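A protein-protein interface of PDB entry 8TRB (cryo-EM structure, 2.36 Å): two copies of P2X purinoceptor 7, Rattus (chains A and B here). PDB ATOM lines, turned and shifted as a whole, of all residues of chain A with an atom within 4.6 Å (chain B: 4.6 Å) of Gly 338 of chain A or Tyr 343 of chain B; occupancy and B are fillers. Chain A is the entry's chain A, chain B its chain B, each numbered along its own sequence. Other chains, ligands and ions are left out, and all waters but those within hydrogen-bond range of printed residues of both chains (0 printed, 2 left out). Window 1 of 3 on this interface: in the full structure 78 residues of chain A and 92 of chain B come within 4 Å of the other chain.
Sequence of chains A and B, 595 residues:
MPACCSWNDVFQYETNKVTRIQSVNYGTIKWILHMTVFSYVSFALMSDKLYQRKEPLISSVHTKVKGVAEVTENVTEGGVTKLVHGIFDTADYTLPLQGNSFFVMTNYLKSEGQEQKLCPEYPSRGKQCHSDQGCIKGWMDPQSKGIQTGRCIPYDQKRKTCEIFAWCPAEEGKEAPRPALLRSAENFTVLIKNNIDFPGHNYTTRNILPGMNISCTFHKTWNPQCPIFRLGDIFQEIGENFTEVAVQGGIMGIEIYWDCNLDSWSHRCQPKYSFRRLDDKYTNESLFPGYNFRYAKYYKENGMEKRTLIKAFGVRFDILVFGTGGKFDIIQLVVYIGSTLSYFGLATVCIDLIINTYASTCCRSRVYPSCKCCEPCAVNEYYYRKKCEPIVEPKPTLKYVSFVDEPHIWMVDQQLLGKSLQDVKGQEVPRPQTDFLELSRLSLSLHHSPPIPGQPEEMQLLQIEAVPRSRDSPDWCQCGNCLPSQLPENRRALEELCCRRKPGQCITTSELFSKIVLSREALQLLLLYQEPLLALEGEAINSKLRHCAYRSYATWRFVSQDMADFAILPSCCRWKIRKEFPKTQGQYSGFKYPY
Printed residues of chain A that touch a printed residue of chain B: Val 334, Val 335, Ile 337, Gly 338, Ser 339, Leu 341 and Ser 342. Hydrophobic or aromatic side chains of chain A that line the printed part of chain B: Val 334, Val 335, Ile 337 and Leu 341. Printed residues of chain B that touch a printed residue of chain A: Ser 339, Ser 342 and Tyr 343. Among the printed residues, 9 pairs touch across the chains.
The backbone carbonyl oxygen (O) of Val 335 of chain A lies close to the side-chain hydroxyl (OG) of Ser 339 of chain A (3.4 Å). OG of Ser 339 of chain A is in hydrogen-bond range of O of Tyr 336 of chain A, at 2.4 Å. O of Ile 337 of chain A lies within hydrogen-bond range of OG1 of Thr 340 of chain A, 3.1 Å away.
Of the printed residues of chain B, Val 334 of chain A touches Tyr 343. Of the printed residues of chain B, Ser 339 of chain A touches Ser 339 (3.5 Å). Of the printed residues of chain A, Ser 339 of chain B touches Val 335 (3.8 Å), Gly 338 (2.9 Å) and Ser 339 (3.5 Å). Printed residues of chain A within 4 Å of Ser 342 of chain B: Leu 341 and Ser 342. Tyr 343 of chain B touches four residues of chain A. Gly 345 of chain B touches none of the printed residues of chain A. The nearest residue of chain B that does not touch Gly 338 of chain A is Ser 342 of chain B (4.2 Å). The nearest printed residue of chain B that does not touch Val 334 of chain A is Ser 339 of chain B (5.2 Å).
Ser 339 of chain A touches its own counterpart, Ser 339 of chain B. Leu 341 of chain A touches Ser 342 of chain B, but with the chains exchanged Ser 342 of chain A does not touch Leu 341 of chain B (6.9 Å). Ser 342 of chain A touches its own counterpart, Ser 342 of chain B. 4 positions are printed for both chains.
O of Val 334 of chain A is in hydrogen-bond range of OH of Tyr 343 of chain B (2.7 Å). The backbone NH of Gly 338 of chain A is in hydrogen-bond range of the side-chain hydroxyl of Tyr 343 of chain B, at 3.3 Å. The backbone NH of Ser 339 of chain A lies within hydrogen-bond range of the backbone carbonyl oxygen of Ser 339 of chain B. The side-chain hydroxyl of Ser 342 of chain A lies within hydrogen-bond range of the side-chain hydroxyl of Ser 342 of chain B. O of Ser 339 of chain B sits close to O of Gly 338 of chain A (3.1 Å).
CB of Ser 339 of chain B touches O of Val 335 of chain A, 3.8 Å away. CG2 of Ile 337 of chain A touches OH of Tyr 343 of chain B, at 3.2 Å. Leu 341 of chain A touches Ser 342 of chain B. Tyr 343 of chain B touches Leu 341 of chain A.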
ATOM      1  N   VAL A 334      -3.960 -28.805  27.660  1.00  0.00           N
ATOM      2  CA  VAL A 334      -2.948 -27.922  27.094  1.00  0.00           C
ATOM      3  C   VAL A 334      -2.058 -27.362  28.193  1.00  0.00           C
ATOM      4  O   VAL A 334      -0.833 -27.298  28.049  1.00  0.00           O
ATOM      5  CB  VAL A 334      -3.627 -26.802  26.282  1.00  0.00           C
ATOM      6  CG1 VAL A 334      -2.660 -25.687  25.978  1.00  0.00           C
ATOM      7  CG2 VAL A 334      -4.204 -27.361  25.008  1.00  0.00           C
ATOM      8  N   VAL A 335      -2.661 -26.950  29.309  1.00  0.00           N
ATOM      9  CA  VAL A 335      -1.890 -26.428  30.429  1.00  0.00           C
ATOM     10  C   VAL A 335      -0.977 -27.503  30.999  1.00  0.00           C
ATOM     11  O   VAL A 335       0.184 -27.235  31.329  1.00  0.00           O
ATOM     12  CB  VAL A 335      -2.837 -25.848  31.494  1.00  0.00           C
ATOM     13  CG1 VAL A 335      -2.106 -25.583  32.783  1.00  0.00           C
ATOM     14  CG2 VAL A 335      -3.472 -24.577  30.990  1.00  0.00           C
ATOM     15  N   TYR A 336      -1.472 -28.737  31.123  1.00  0.00           N
ATOM     16  CA  TYR A 336      -0.625 -29.810  31.633  1.00  0.00           C
ATOM     17  C   TYR A 336       0.538 -30.103  30.691  1.00  0.00           C
ATOM     18  O   TYR A 336       1.682 -30.280  31.134  1.00  0.00           O
ATOM     19  CB  TYR A 336      -1.448 -31.077  31.860  1.00  0.00           C
ATOM     20  CG  TYR A 336      -0.601 -32.270  32.204  1.00  0.00           C
ATOM     21  CD1 TYR A 336      -0.107 -32.437  33.480  1.00  0.00           C
ATOM     22  CD2 TYR A 336      -0.271 -33.214  31.249  1.00  0.00           C
ATOM     23  CE1 TYR A 336       0.674 -33.509  33.798  1.00  0.00           C
ATOM     24  CE2 TYR A 336       0.507 -34.289  31.563  1.00  0.00           C
ATOM     25  CZ  TYR A 336       0.978 -34.434  32.839  1.00  0.00           C
ATOM     26  OH  TYR A 336       1.761 -35.510  33.160  1.00  0.00           O
ATOM     27  N   ILE A 337       0.263 -30.174  29.387  1.00  0.00           N
ATOM     28  CA  ILE A 337       1.315 -30.455  28.419  1.00  0.00           C
ATOM     29  C   ILE A 337       2.356 -29.345  28.440  1.00  0.00           C
ATOM     30  O   ILE A 337       3.561 -29.605  28.378  1.00  0.00           O
ATOM     31  CB  ILE A 337       0.710 -30.653  27.016  1.00  0.00           C
ATOM     32  CG1 ILE A 337      -0.024 -31.989  26.944  1.00  0.00           C
ATOM     33  CG2 ILE A 337       1.780 -30.594  25.945  1.00  0.00           C
ATOM     34  CD1 ILE A 337      -0.965 -32.097  25.791  1.00  0.00           C
ATOM     35  N   GLY A 338       1.908 -28.095  28.528  1.00  0.00           N
ATOM     36  CA  GLY A 338       2.841 -26.993  28.646  1.00  0.00           C
ATOM     37  C   GLY A 338       3.669 -27.059  29.914  1.00  0.00           C
ATOM     38  O   GLY A 338       4.859 -26.745  29.906  1.00  0.00           O
ATOM     39  N   SER A 339       3.043 -27.457  31.019  1.00  0.00           N
ATOM     40  CA  SER A 339       3.761 -27.588  32.279  1.00  0.00           C
ATOM     41  C   SER A 339       4.833 -28.663  32.191  1.00  0.00           C
ATOM     42  O   SER A 339       5.894 -28.545  32.810  1.00  0.00           O
ATOM     43  CB  SER A 339       2.782 -27.905  33.406  1.00  0.00           C
ATOM     44  OG  SER A 339       2.218 -29.191  33.241  1.00  0.00           O
ATOM     45  N   THR A 340       4.574 -29.720  31.435  1.00  0.00           N
ATOM     46  CA  THR A 340       5.504 -30.838  31.374  1.00  0.00           C
ATOM     47  C   THR A 340       6.481 -30.764  30.204  1.00  0.00           C
ATOM     48  O   THR A 340       7.416 -31.568  30.152  1.00  0.00           O
ATOM     49  CB  THR A 340       4.729 -32.156  31.303  1.00  0.00           C
ATOM     50  OG1 THR A 340       3.747 -32.089  30.268  1.00  0.00           O
ATOM     51  CG2 THR A 340       4.038 -32.431  32.618  1.00  0.00           C
ATOM     52  N   LEU A 341       6.297 -29.822  29.280  1.00  0.00           N
ATOM     53  CA  LEU A 341       7.157 -29.756  28.101  1.00  0.00           C
ATOM     54  C   LEU A 341       8.617 -29.537  28.477  1.00  0.00           C
ATOM     55  O   LEU A 341       9.516 -30.130  27.869  1.00  0.00           O
ATOM     56  CB  LEU A 341       6.679 -28.642  27.176  1.00  0.00           C
ATOM     57  CG  LEU A 341       5.678 -29.018  26.086  1.00  0.00           C
ATOM     58  CD1 LEU A 341       5.184 -27.777  25.367  1.00  0.00           C
ATOM     59  CD2 LEU A 341       6.272 -30.012  25.125  1.00  0.00           C
ATOM     60  N   SER A 342       8.877 -28.676  29.459  1.00  0.00           N
ATOM     61  CA  SER A 342      10.249 -28.366  29.833  1.00  0.00           C
ATOM     62  C   SER A 342      11.001 -29.569  30.381  1.00  0.00           C
ATOM     63  O   SER A 342      12.233 -29.538  30.436  1.00  0.00           O
ATOM     64  CB  SER A 342      10.267 -27.237  30.855  1.00  0.00           C
ATOM     65  OG  SER A 342      10.233 -25.981  30.218  1.00  0.00           O
ATOM     66  N   VAL B  37      -0.167 -18.732  19.098  1.00  0.00           N
ATOM     67  CA  VAL B  37       0.050 -19.237  20.450  1.00  0.00           C
ATOM     68  C   VAL B  37      -0.354 -18.187  21.473  1.00  0.00           C
ATOM     69  O   VAL B  37      -1.028 -18.491  22.465  1.00  0.00           O
ATOM     70  CB  VAL B  37       1.517 -19.669  20.632  1.00  0.00           C
ATOM     71  CG1 VAL B  37       1.816 -19.971  22.082  1.00  0.00           C
ATOM     72  CG2 VAL B  37       1.828 -20.869  19.775  1.00  0.00           C
ATOM     73  N   SER B 339       3.449 -22.322  32.604  1.00  0.00           N
ATOM     74  CA  SER B 339       2.959 -23.524  31.943  1.00  0.00           C
ATOM     75  C   SER B 339       2.860 -23.322  30.440  1.00  0.00           C
ATOM     76  O   SER B 339       3.081 -24.256  29.665  1.00  0.00           O
ATOM     77  CB  SER B 339       1.601 -23.917  32.518  1.00  0.00           C
ATOM     78  OG  SER B 339       0.614 -22.961  32.185  1.00  0.00           O
ATOM     79  N   THR B 340       2.523 -22.116  30.008  1.00  0.00           N
ATOM     80  CA  THR B 340       2.309 -21.863  28.591  1.00  0.00           C
ATOM     81  C   THR B 340       3.540 -21.317  27.871  1.00  0.00           C
ATOM     82  O   THR B 340       3.524 -21.227  26.640  1.00  0.00           O
ATOM     83  CB  THR B 340       1.143 -20.892  28.404  1.00  0.00           C
ATOM     84  OG1 THR B 340       1.327 -19.743  29.234  1.00  0.00           O
ATOM     85  CG2 THR B 340      -0.161 -21.559  28.774  1.00  0.00           C
ATOM     86  N   LEU B 341       4.600 -20.970  28.597  1.00  0.00           N
ATOM     87  CA  LEU B 341       5.773 -20.370  27.966  1.00  0.00           C
ATOM     88  C   LEU B 341       6.401 -21.304  26.937  1.00  0.00           C
ATOM     89  O   LEU B 341       6.833 -20.858  25.868  1.00  0.00           O
ATOM     90  CB  LEU B 341       6.798 -19.998  29.031  1.00  0.00           C
ATOM     91  CG  LEU B 341       6.728 -18.585  29.605  1.00  0.00           C
ATOM     92  CD1 LEU B 341       7.702 -18.432  30.759  1.00  0.00           C
ATOM     93  CD2 LEU B 341       6.973 -17.553  28.538  1.00  0.00           C
ATOM     94  N   SER B 342       6.478 -22.596  27.246  1.00  0.00           N
ATOM     95  CA  SER B 342       7.121 -23.541  26.343  1.00  0.00           C
ATOM     96  C   SER B 342       6.400 -23.669  25.009  1.00  0.00           C
ATOM     97  O   SER B 342       6.991 -24.173  24.050  1.00  0.00           O
ATOM     98  CB  SER B 342       7.225 -24.908  27.007  1.00  0.00           C
ATOM     99  OG  SER B 342       8.383 -24.992  27.803  1.00  0.00           O
ATOM    100  N   TYR B 343       5.143 -23.235  24.921  1.00  0.00           N
ATOM    101  CA  TYR B 343       4.430 -23.307  23.654  1.00  0.00           C
ATOM    102  C   TYR B 343       4.941 -22.287  22.648  1.00  0.00           C
ATOM    103  O   TYR B 343       4.636 -22.401  21.458  1.00  0.00           O
ATOM    104  CB  TYR B 343       2.933 -23.115  23.876  1.00  0.00           C
ATOM    105  CG  TYR B 343       2.222 -24.357  24.346  1.00  0.00           C
ATOM    106  CD1 TYR B 343       2.260 -25.522  23.602  1.00  0.00           C
ATOM    107  CD2 TYR B 343       1.507 -24.364  25.530  1.00  0.00           C
ATOM    108  CE1 TYR B 343       1.616 -26.655  24.026  1.00  0.00           C
ATOM    109  CE2 TYR B 343       0.862 -25.486  25.955  1.00  0.00           C
ATOM    110  CZ  TYR B 343       0.917 -26.630  25.204  1.00  0.00           C
ATOM    111  OH  TYR B 343       0.264 -27.752  25.640  1.00  0.00           O
ATOM    112  N   PHE B 344       5.710 -21.299  23.096  1.00  0.00           N
ATOM    113  CA  PHE B 344       6.263 -20.296  22.200  1.00  0.00           C
ATOM    114  C   PHE B 344       7.481 -20.794  21.434  1.00  0.00           C
ATOM    115  O   PHE B 344       7.968 -20.082  20.552  1.00  0.00           O
ATOM    116  CB  PHE B 344       6.610 -19.038  22.993  1.00  0.00           C
ATOM    117  CG  PHE B 344       5.411 -18.248  23.414  1.00  0.00           C
ATOM    118  CD1 PHE B 344       4.763 -17.422  22.519  1.00  0.00           C
ATOM    119  CD2 PHE B 344       4.919 -18.343  24.702  1.00  0.00           C
ATOM    120  CE1 PHE B 344       3.659 -16.703  22.900  1.00  0.00           C
ATOM    121  CE2 PHE B 344       3.817 -17.627  25.086  1.00  0.00           C
ATOM    122  CZ  PHE B 344       3.185 -16.806  24.186  1.00  0.00           C
ATOM    123  N   GLY B 345       7.978 -21.986  21.743  1.00  0.00           N
ATOM    124  CA  GLY B 345       8.957 -22.671  20.930  1.00  0.00           C
ATOM    125  C   GLY B 345       8.393 -23.434  19.759  1.00  0.00           C
ATOM    126  O   GLY B 345       9.139 -24.113  19.048  1.00  0.00           O
ATOM    127  N   LEU B 346       7.078 -23.347  19.550  1.00  0.00           N
ATOM    128  CA  LEU B 346       6.445 -24.056  18.447  1.00  0.00           C
ATOM    129  C   LEU B 346       6.987 -23.593  17.104  1.00  0.00           C
ATOM    130  O   LEU B 346       7.240 -24.412  16.215  1.00  0.00           O
ATOM    131  CB  LEU B 346       4.930 -23.855  18.508  1.00  0.00           C
ATOM    132  CG  LEU B 346       4.114 -24.328  17.307  1.00  0.00           C
ATOM    133  CD1 LEU B 346       4.039 -25.835  17.314  1.00  0.00           C
ATOM    134  CD2 LEU B 346       2.734 -23.724  17.316  1.00  0.00           C
